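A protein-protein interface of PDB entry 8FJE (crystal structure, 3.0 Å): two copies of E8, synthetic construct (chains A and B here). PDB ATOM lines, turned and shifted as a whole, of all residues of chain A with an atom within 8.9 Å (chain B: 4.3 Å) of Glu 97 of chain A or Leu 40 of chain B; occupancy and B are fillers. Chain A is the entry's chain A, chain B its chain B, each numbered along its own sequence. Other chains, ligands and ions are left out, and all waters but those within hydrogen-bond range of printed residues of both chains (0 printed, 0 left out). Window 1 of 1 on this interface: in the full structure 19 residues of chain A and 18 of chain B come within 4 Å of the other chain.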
ATOM      1  N   GLU A  69      20.574 -35.131   9.482  1.00  0.00           N
ATOM      2  CA  GLU A  69      20.802 -34.324   8.288  1.00  0.00           C
ATOM      3  C   GLU A  69      21.043 -35.168   7.043  1.00  0.00           C
ATOM      4  O   GLU A  69      20.970 -34.632   5.932  1.00  0.00           O
ATOM      5  CB  GLU A  69      21.981 -33.375   8.504  1.00  0.00           C
ATOM      6  CG  GLU A  69      23.341 -34.047   8.469  1.00  0.00           C
ATOM      7  CD  GLU A  69      23.853 -34.391   9.853  1.00  0.00           C
ATOM      8  OE1 GLU A  69      23.053 -34.345  10.811  1.00  0.00           O
ATOM      9  OE2 GLU A  69      25.054 -34.706   9.982  1.00  0.00           O
ATOM     10  N   GLU A  72      17.221 -37.231   6.319  1.00  0.00           N
ATOM     11  CA  GLU A  72      16.332 -36.350   5.570  1.00  0.00           C
ATOM     12  C   GLU A  72      16.833 -36.138   4.148  1.00  0.00           C
ATOM     13  O   GLU A  72      16.034 -36.053   3.209  1.00  0.00           O
ATOM     14  CB  GLU A  72      16.191 -35.012   6.298  1.00  0.00           C
ATOM     15  CG  GLU A  72      15.549 -33.898   5.478  1.00  0.00           C
ATOM     16  CD  GLU A  72      14.061 -34.105   5.248  1.00  0.00           C
ATOM     17  OE1 GLU A  72      13.682 -35.071   4.553  1.00  0.00           O
ATOM     18  OE2 GLU A  72      13.266 -33.293   5.766  1.00  0.00           O
ATOM     19  N   ARG A  73      18.154 -36.053   3.969  1.00  0.00           N
ATOM     20  CA  ARG A  73      18.713 -35.877   2.632  1.00  0.00           C
ATOM     21  C   ARG A  73      18.301 -37.018   1.711  1.00  0.00           C
ATOM     22  O   ARG A  73      17.854 -36.790   0.582  1.00  0.00           O
ATOM     23  CB  ARG A  73      20.236 -35.770   2.708  1.00  0.00           C
ATOM     24  CG  ARG A  73      20.919 -35.796   1.348  1.00  0.00           C
ATOM     25  CD  ARG A  73      22.432 -35.817   1.482  1.00  0.00           C
ATOM     26  NE  ARG A  73      22.952 -34.574   2.039  1.00  0.00           N
ATOM     27  CZ  ARG A  73      23.233 -33.495   1.322  1.00  0.00           C
ATOM     28  NH1 ARG A  73      23.055 -33.470   0.011  1.00  0.00           N
ATOM     29  NH2 ARG A  73      23.706 -32.413   1.935  1.00  0.00           N
ATOM     30  N   LEU A  76      14.477 -37.072   0.810  1.00  0.00           N
ATOM     31  CA  LEU A  76      14.129 -36.151  -0.265  1.00  0.00           C
ATOM     32  C   LEU A  76      14.691 -36.625  -1.599  1.00  0.00           C
ATOM     33  O   LEU A  76      14.041 -36.472  -2.639  1.00  0.00           O
ATOM     34  CB  LEU A  76      14.628 -34.747   0.069  1.00  0.00           C
ATOM     35  CG  LEU A  76      14.144 -34.214   1.418  1.00  0.00           C
ATOM     36  CD1 LEU A  76      14.745 -32.857   1.701  1.00  0.00           C
ATOM     37  CD2 LEU A  76      12.626 -34.145   1.451  1.00  0.00           C
ATOM     38  N   THR A  93      23.282 -33.175  -6.625  1.00  0.00           N
ATOM     39  CA  THR A  93      23.937 -31.875  -6.544  1.00  0.00           C
ATOM     40  C   THR A  93      23.082 -30.816  -5.861  1.00  0.00           C
ATOM     41  O   THR A  93      23.633 -29.859  -5.304  1.00  0.00           O
ATOM     42  CB  THR A  93      24.321 -31.384  -7.943  1.00  0.00           C
ATOM     43  OG1 THR A  93      23.166 -30.841  -8.595  1.00  0.00           O
ATOM     44  CG2 THR A  93      24.885 -32.526  -8.774  1.00  0.00           C
ATOM     45  N   MET A  94      21.761 -30.956  -5.896  1.00  0.00           N
ATOM     46  CA  MET A  94      20.895 -29.990  -5.235  1.00  0.00           C
ATOM     47  C   MET A  94      21.141 -30.014  -3.729  1.00  0.00           C
ATOM     48  O   MET A  94      21.192 -31.098  -3.130  1.00  0.00           O
ATOM     49  CB  MET A  94      19.424 -30.284  -5.531  1.00  0.00           C
ATOM     50  CG  MET A  94      19.007 -30.008  -6.967  1.00  0.00           C
ATOM     51  SD  MET A  94      17.251 -30.284  -7.283  1.00  0.00           S
ATOM     52  CE  MET A  94      16.657 -30.736  -5.655  1.00  0.00           C
ATOM     53  N   PRO A  95      21.301 -28.859  -3.089  1.00  0.00           N
ATOM     54  CA  PRO A  95      21.539 -28.838  -1.642  1.00  0.00           C
ATOM     55  C   PRO A  95      20.307 -29.288  -0.871  1.00  0.00           C
ATOM     56  O   PRO A  95      19.215 -29.460  -1.417  1.00  0.00           O
ATOM     57  CB  PRO A  95      21.876 -27.371  -1.357  1.00  0.00           C
ATOM     58  CG  PRO A  95      21.210 -26.617  -2.463  1.00  0.00           C
ATOM     59  CD  PRO A  95      21.299 -27.505  -3.670  1.00  0.00           C
ATOM     60  N   LEU A  96      20.504 -29.480   0.436  1.00  0.00           N
ATOM     61  CA  LEU A  96      19.419 -29.955   1.288  1.00  0.00           C
ATOM     62  C   LEU A  96      18.289 -28.936   1.366  1.00  0.00           C
ATOM     63  O   LEU A  96      17.109 -29.307   1.367  1.00  0.00           O
ATOM     64  CB  LEU A  96      19.955 -30.275   2.684  1.00  0.00           C
ATOM     65  CG  LEU A  96      18.977 -30.901   3.681  1.00  0.00           C
ATOM     66  CD1 LEU A  96      18.210 -32.045   3.035  1.00  0.00           C
ATOM     67  CD2 LEU A  96      19.713 -31.382   4.923  1.00  0.00           C
ATOM     68  N   GLU A  97      18.627 -27.646   1.429  1.00  0.00           N
ATOM     69  CA  GLU A  97      17.597 -26.615   1.492  1.00  0.00           C
ATOM     70  C   GLU A  97      16.797 -26.541   0.198  1.00  0.00           C
ATOM     71  O   GLU A  97      15.614 -26.181   0.221  1.00  0.00           O
ATOM     72  CB  GLU A  97      18.225 -25.258   1.810  1.00  0.00           C
ATOM     73  CG  GLU A  97      18.439 -25.005   3.297  1.00  0.00           C
ATOM     74  CD  GLU A  97      19.531 -25.874   3.898  1.00  0.00           C
ATOM     75  OE1 GLU A  97      20.343 -26.438   3.133  1.00  0.00           O
ATOM     76  OE2 GLU A  97      19.573 -25.993   5.141  1.00  0.00           O
ATOM     77  N   GLU A  98      17.416 -26.875  -0.934  1.00  0.00           N
ATOM     78  CA  GLU A  98      16.683 -26.930  -2.191  1.00  0.00           C
ATOM     79  C   GLU A  98      15.969 -28.260  -2.383  1.00  0.00           C
ATOM     80  O   GLU A  98      14.976 -28.316  -3.116  1.00  0.00           O
ATOM     81  CB  GLU A  98      17.626 -26.671  -3.367  1.00  0.00           C
ATOM     82  CG  GLU A  98      17.758 -25.201  -3.745  1.00  0.00           C
ATOM     83  CD  GLU A  98      16.421 -24.553  -4.053  1.00  0.00           C
ATOM     84  OE1 GLU A  98      15.779 -24.027  -3.119  1.00  0.00           O
ATOM     85  OE2 GLU A  98      16.003 -24.580  -5.230  1.00  0.00           O
ATOM     86  N   LEU A  99      16.453 -29.328  -1.744  1.00  0.00           N
ATOM     87  CA  LEU A  99      15.726 -30.591  -1.766  1.00  0.00           C
ATOM     88  C   LEU A  99      14.396 -30.468  -1.033  1.00  0.00           C
ATOM     89  O   LEU A  99      13.391 -31.050  -1.458  1.00  0.00           O
ATOM     90  CB  LEU A  99      16.582 -31.699  -1.152  1.00  0.00           C
ATOM     91  CG  LEU A  99      17.631 -32.362  -2.047  1.00  0.00           C
ATOM     92  CD1 LEU A  99      18.651 -33.116  -1.208  1.00  0.00           C
ATOM     93  CD2 LEU A  99      16.961 -33.301  -3.036  1.00  0.00           C
ATOM     94  N   GLU A 100      14.370 -29.711   0.068  1.00  0.00           N
ATOM     95  CA  GLU A 100      13.123 -29.514   0.804  1.00  0.00           C
ATOM     96  C   GLU A 100      12.137 -28.672   0.006  1.00  0.00           C
ATOM     97  O   GLU A 100      10.926 -28.915   0.051  1.00  0.00           O
ATOM     98  CB  GLU A 100      13.404 -28.853   2.155  1.00  0.00           C
ATOM     99  CG  GLU A 100      14.341 -29.631   3.064  1.00  0.00           C
ATOM    100  CD  GLU A 100      14.257 -29.184   4.512  1.00  0.00           C
ATOM    101  OE1 GLU A 100      13.296 -28.466   4.859  1.00  0.00           O
ATOM    102  OE2 GLU A 100      15.154 -29.551   5.302  1.00  0.00           O
ATOM    103  N   ARG A 101      12.636 -27.674  -0.727  1.00  0.00           N
ATOM    104  CA  ARG A 101      11.748 -26.771  -1.452  1.00  0.00           C
ATOM    105  C   ARG A 101      11.040 -27.494  -2.591  1.00  0.00           C
ATOM    106  O   ARG A 101       9.812 -27.425  -2.713  1.00  0.00           O
ATOM    107  CB  ARG A 101      12.535 -25.573  -1.980  1.00  0.00           C
ATOM    108  CG  ARG A 101      11.672 -24.521  -2.650  1.00  0.00           C
ATOM    109  CD  ARG A 101      12.515 -23.440  -3.303  1.00  0.00           C
ATOM    110  NE  ARG A 101      12.469 -22.188  -2.554  1.00  0.00           N
ATOM    111  CZ  ARG A 101      11.450 -21.340  -2.567  1.00  0.00           C
ATOM    112  NH1 ARG A 101      10.356 -21.582  -3.271  1.00  0.00           N
ATOM    113  NH2 ARG A 101      11.528 -20.222  -1.852  1.00  0.00           N
ATOM    114  N   GLU A 102      11.799 -28.196  -3.434  1.00  0.00           N
ATOM    115  CA  GLU A 102      11.195 -28.901  -4.557  1.00  0.00           C
ATOM    116  C   GLU A 102      10.376 -30.105  -4.111  1.00  0.00           C
ATOM    117  O   GLU A 102       9.470 -30.524  -4.839  1.00  0.00           O
ATOM    118  CB  GLU A 102      12.277 -29.336  -5.549  1.00  0.00           C
ATOM    119  CG  GLU A 102      13.158 -28.198  -6.063  1.00  0.00           C
ATOM    120  CD  GLU A 102      12.483 -27.335  -7.121  1.00  0.00           C
ATOM    121  OE1 GLU A 102      11.328 -26.903  -6.912  1.00  0.00           O
ATOM    122  OE2 GLU A 102      13.114 -27.085  -8.169  1.00  0.00           O
ATOM    123  N   ALA A 103      10.669 -30.668  -2.937  1.00  0.00           N
ATOM    124  CA  ALA A 103       9.832 -31.740  -2.407  1.00  0.00           C
ATOM    125  C   ALA A 103       8.510 -31.196  -1.886  1.00  0.00           C
ATOM    126  O   ALA A 103       7.464 -31.839  -2.038  1.00  0.00           O
ATOM    127  CB  ALA A 103      10.568 -32.490  -1.297  1.00  0.00           C
ATOM    128  N   LEU A 104       8.535 -30.015  -1.265  1.00  0.00           N
ATOM    129  CA  LEU A 104       7.305 -29.437  -0.734  1.00  0.00           C
ATOM    130  C   LEU A 104       6.399 -28.943  -1.854  1.00  0.00           C
ATOM    131  O   LEU A 104       5.174 -29.091  -1.778  1.00  0.00           O
ATOM    132  CB  LEU A 104       7.632 -28.304   0.236  1.00  0.00           C
ATOM    133  CG  LEU A 104       7.760 -28.662   1.720  1.00  0.00           C
ATOM    134  CD1 LEU A 104       8.453 -30.002   1.930  1.00  0.00           C
ATOM    135  CD2 LEU A 104       8.505 -27.559   2.444  1.00  0.00           C
ATOM    136  N   PRO A 123       7.592 -18.686   0.334  1.00  0.00           N
ATOM    137  CA  PRO A 123       8.948 -19.077   0.728  1.00  0.00           C
ATOM    138  C   PRO A 123       8.942 -20.480   1.330  1.00  0.00           C
ATOM    139  O   PRO A 123       7.899 -21.109   1.495  1.00  0.00           O
ATOM    140  CB  PRO A 123       9.333 -18.016   1.760  1.00  0.00           C
ATOM    141  CG  PRO A 123       8.038 -17.595   2.354  1.00  0.00           C
ATOM    142  CD  PRO A 123       7.020 -17.677   1.245  1.00  0.00           C
ATOM    143  N   LEU A 124      10.142 -20.963   1.661  1.00  0.00           N
ATOM    144  CA  LEU A 124      10.272 -22.323   2.177  1.00  0.00           C
ATOM    145  C   LEU A 124       9.630 -22.475   3.551  1.00  0.00           C
ATOM    146  O   LEU A 124       9.144 -23.560   3.888  1.00  0.00           O
ATOM    147  CB  LEU A 124      11.746 -22.726   2.229  1.00  0.00           C
ATOM    148  CG  LEU A 124      12.056 -24.163   2.658  1.00  0.00           C
ATOM    149  CD1 LEU A 124      11.282 -25.150   1.803  1.00  0.00           C
ATOM    150  CD2 LEU A 124      13.549 -24.435   2.574  1.00  0.00           C
ATOM    151  N   GLU A 125       9.612 -21.406   4.351  1.00  0.00           N
ATOM    152  CA  GLU A 125       8.996 -21.489   5.672  1.00  0.00           C
ATOM    153  C   GLU A 125       7.489 -21.686   5.580  1.00  0.00           C
ATOM    154  O   GLU A 125       6.896 -22.331   6.452  1.00  0.00           O
ATOM    155  CB  GLU A 125       9.311 -20.231   6.480  1.00  0.00           C
ATOM    156  CG  GLU A 125       9.181 -18.938   5.691  1.00  0.00           C
ATOM    157  CD  GLU A 125       9.220 -17.710   6.579  1.00  0.00           C
ATOM    158  OE1 GLU A 125       8.390 -17.622   7.507  1.00  0.00           O
ATOM    159  OE2 GLU A 125      10.078 -16.833   6.346  1.00  0.00           O
ATOM    160  N   LEU A 127       5.836 -22.929   2.647  1.00  0.00           N
ATOM    161  CA  LEU A 127       5.534 -24.158   1.920  1.00  0.00           C
ATOM    162  C   LEU A 127       5.396 -25.342   2.867  1.00  0.00           C
ATOM    163  O   LEU A 127       4.608 -26.259   2.606  1.00  0.00           O
ATOM    164  CB  LEU A 127       6.622 -24.440   0.882  1.00  0.00           C
ATOM    165  CG  LEU A 127       6.549 -23.701  -0.456  1.00  0.00           C
ATOM    166  CD1 LEU A 127       7.892 -23.757  -1.167  1.00  0.00           C
ATOM    167  CD2 LEU A 127       5.453 -24.277  -1.335  1.00  0.00           C
ATOM    168  N   GLU B  13      14.778 -18.330   5.287  1.00  0.00           N
ATOM    169  CA  GLU B  13      15.915 -19.036   4.704  1.00  0.00           C
ATOM    170  C   GLU B  13      17.049 -18.080   4.355  1.00  0.00           C
ATOM    171  O   GLU B  13      18.217 -18.483   4.353  1.00  0.00           O
ATOM    172  CB  GLU B  13      15.470 -19.820   3.468  1.00  0.00           C
ATOM    173  CG  GLU B  13      15.042 -18.959   2.291  1.00  0.00           C
ATOM    174  CD  GLU B  13      13.763 -19.452   1.642  1.00  0.00           C
ATOM    175  OE1 GLU B  13      12.777 -19.680   2.372  1.00  0.00           O
ATOM    176  OE2 GLU B  13      13.746 -19.617   0.403  1.00  0.00           O
ATOM    177  N   ARG B  17      20.936 -17.603   6.380  1.00  0.00           N
ATOM    178  CA  ARG B  17      22.135 -17.581   5.549  1.00  0.00           C
ATOM    179  C   ARG B  17      23.002 -16.368   5.864  1.00  0.00           C
ATOM    180  O   ARG B  17      24.211 -16.498   6.090  1.00  0.00           O
ATOM    181  CB  ARG B  17      21.743 -17.594   4.072  1.00  0.00           C
ATOM    182  CG  ARG B  17      22.809 -18.146   3.144  1.00  0.00           C
ATOM    183  CD  ARG B  17      22.418 -17.929   1.692  1.00  0.00           C
ATOM    184  NE  ARG B  17      20.995 -18.160   1.476  1.00  0.00           N
ATOM    185  CZ  ARG B  17      20.497 -19.147   0.744  1.00  0.00           C
ATOM    186  NH1 ARG B  17      21.282 -20.018   0.132  1.00  0.00           N
ATOM    187  NH2 ARG B  17      19.177 -19.260   0.619  1.00  0.00           N
ATOM    188  N   MET B  38      28.867 -21.701  -0.266  1.00  0.00           N
ATOM    189  CA  MET B  38      28.693 -22.922   0.504  1.00  0.00           C
ATOM    190  C   MET B  38      27.211 -23.198   0.758  1.00  0.00           C
ATOM    191  O   MET B  38      26.414 -22.268   0.907  1.00  0.00           O
ATOM    192  CB  MET B  38      29.430 -22.824   1.835  1.00  0.00           C
ATOM    193  CG  MET B  38      30.924 -22.570   1.714  1.00  0.00           C
ATOM    194  SD  MET B  38      31.817 -23.954   0.976  1.00  0.00           S
ATOM    195  CE  MET B  38      32.098 -23.352  -0.687  1.00  0.00           C
ATOM    196  N   PRO B  39      26.818 -24.470   0.811  1.00  0.00           N
ATOM    197  CA  PRO B  39      25.429 -24.794   1.145  1.00  0.00           C
ATOM    198  C   PRO B  39      25.126 -24.471   2.598  1.00  0.00           C
ATOM    199  O   PRO B  39      25.998 -24.530   3.468  1.00  0.00           O
ATOM    200  CB  PRO B  39      25.341 -26.300   0.877  1.00  0.00           C
ATOM    201  CG  PRO B  39      26.737 -26.786   1.074  1.00  0.00           C
ATOM    202  CD  PRO B  39      27.625 -25.679   0.572  1.00  0.00           C
ATOM    203  N   LEU B  40      23.862 -24.123   2.854  1.00  0.00           N
ATOM    204  CA  LEU B  40      23.467 -23.710   4.197  1.00  0.00           C
ATOM    205  C   LEU B  40      23.623 -24.840   5.206  1.00  0.00           C
ATOM    206  O   LEU B  40      23.842 -24.580   6.395  1.00  0.00           O
ATOM    207  CB  LEU B  40      22.026 -23.195   4.185  1.00  0.00           C
ATOM    208  CG  LEU B  40      21.603 -22.313   5.362  1.00  0.00           C
ATOM    209  CD1 LEU B  40      20.703 -21.187   4.883  1.00  0.00           C
ATOM    210  CD2 LEU B  40      20.901 -23.137   6.429  1.00  0.00           C
ATOM    211  N   GLU B  41      23.507 -26.093   4.759  1.00  0.00           N
ATOM    212  CA  GLU B  41      23.799 -27.218   5.643  1.00  0.00           C
ATOM    213  C   GLU B  41      25.235 -27.156   6.144  1.00  0.00           C
ATOM    214  O   GLU B  41      25.506 -27.434   7.319  1.00  0.00           O
ATOM    215  CB  GLU B  41      23.543 -28.538   4.916  1.00  0.00           C
ATOM    216  CG  GLU B  41      24.159 -29.752   5.599  1.00  0.00           C
ATOM    217  CD  GLU B  41      24.383 -30.909   4.643  1.00  0.00           C
ATOM    218  OE1 GLU B  41      23.394 -31.573   4.266  1.00  0.00           O
ATOM    219  OE2 GLU B  41      25.549 -31.154   4.270  1.00  0.00           O
ATOM    220  N   GLU B  42      26.168 -26.780   5.269  1.00  0.00           N
ATOM    221  CA  GLU B  42      27.571 -26.706   5.656  1.00  0.00           C
ATOM    222  C   GLU B  42      27.893 -25.417   6.402  1.00  0.00           C
ATOM    223  O   GLU B  42      28.838 -25.391   7.199  1.00  0.00           O
ATOM    224  CB  GLU B  42      28.462 -26.838   4.420  1.00  0.00           C
ATOM    225  CG  GLU B  42      29.909 -27.183   4.731  1.00  0.00           C
ATOM    226  CD  GLU B  42      30.055 -28.525   5.422  1.00  0.00           C
ATOM    227  OE1 GLU B  42      29.234 -29.430   5.155  1.00  0.00           O
ATOM    228  OE2 GLU B  42      30.990 -28.677   6.237  1.00  0.00           O
ATOM    229  N   LEU B  43      27.133 -24.346   6.157  1.00  0.00           N
ATOM    230  CA  LEU B  43      27.353 -23.100   6.884  1.00  0.00           C
ATOM    231  C   LEU B  43      27.191 -23.309   8.386  1.00  0.00           C
ATOM    232  O   LEU B  43      28.026 -22.861   9.179  1.00  0.00           O
ATOM    233  CB  LEU B  43      26.394 -22.017   6.389  1.00  0.00           C
ATOM    234  CG  LEU B  43      26.621 -21.446   4.988  1.00  0.00           C
ATOM    235  CD1 LEU B  43      25.498 -20.489   4.617  1.00  0.00           C
ATOM    236  CD2 LEU B  43      27.966 -20.747   4.909  1.00  0.00           C
ATOM    237  N   GLU B  44      26.121 -23.999   8.791  1.00  0.00           N
ATOM    238  CA  GLU B  44      25.903 -24.257  10.210  1.00  0.00           C
ATOM    239  C   GLU B  44      27.003 -25.139  10.786  1.00  0.00           C
ATOM    240  O   GLU B  44      27.453 -24.923  11.917  1.00  0.00           O
ATOM    241  CB  GLU B  44      24.537 -24.908  10.425  1.00  0.00           C
ATOM    242  CG  GLU B  44      23.406 -24.268   9.641  1.00  0.00           C
ATOM    243  CD  GLU B  44      22.042 -24.738  10.104  1.00  0.00           C
ATOM    244  OE1 GLU B  44      21.944 -25.243  11.242  1.00  0.00           O
ATOM    245  OE2 GLU B  44      21.069 -24.602   9.333  1.00  0.00           O
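Glu 97 of chain A touches just these residues of chain B: Leu 40 (3.4 Å) and Glu 41 (3.6 Å). Of chain A, only Glu 97 comes within 4 Å of Leu 40 of chain B. Printed residues of chain B within 4 Å of Arg 101 of chain A: Glu 13. Printed residues of chain B within 4 Å of Pro 123 of chain A: Glu 13 (3.9 Å). Of the printed residues of chain A, Glu 41 of chain B touches Arg 73, Leu 96 and Glu 97. Printed residues of chain A within 4 Å of Glu 13 of chain B: Arg 101, Pro 123 and Leu 124. Of the printed residues of chain B, Leu 96 of chain A touches Glu 41 (3.7 Å). Glu 98 of chain A touches none of the printed residues of chain B. Pro 95 of chain A touches none of the printed residues of chain B. The nearest printed residue of chain B that does not touch Glu 97 of chain A is Glu 44 of chain B (4.7 Å).
No position is printed for both chains. Of the 7 pairs that touch across the chains among the printed residues, none has its exchanged pair printed and touching as well.
Among the printed residues, merely in contact across the chains: Leu 96 of chain A with Glu 41 of chain B, Glu 97 of chain A with Leu 40 of chain B, Glu 97 of chain A with Glu 41 of chain B and Pro 123 of chain A with Glu 13 of chain B.
The backbone NH (N) of Leu 124 of chain A is in hydrogen-bond range of the side-chain carboxylate (OE1) of Glu 13 of chain B (3.0 Å). The guanidinium group (NH2) of Arg 73 of chain A is in salt-bridge range of the side-chain carboxylate (OE1) of Glu 41 of chain B (2.5 Å). The side-chain carboxylate (OE2) of Glu 13 of chain B is in salt-bridge range of the guanidinium group (NH2) of Arg 101 of chain A (3.2 Å).
The side-chain carboxylate (OE1) of Glu 98 of chain A lies within salt-bridge range of the guanidinium group (NE) of Arg 101 of chain A (3.8 Å).
Printed residues of chain A that touch a printed residue of chain B: Arg 73, Leu 96, Glu 97, Arg 101, Pro 123 and Leu 124. Hydrophobic or aromatic side chains of chain A that line the printed part of chain B: Leu 96, Pro 123 and Leu 124. Along chain A the printed residues that touch a printed residue of chain B span positions 73 to 124. Of the 9 printed residues of chain B, 3 touch a printed residue of chain A. Hydrophobic or aromatic side chains of chain B that line the printed part of chain A: Leu 40. Along chain B the printed residues that touch a printed residue of chain A span positions 13 to 41.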
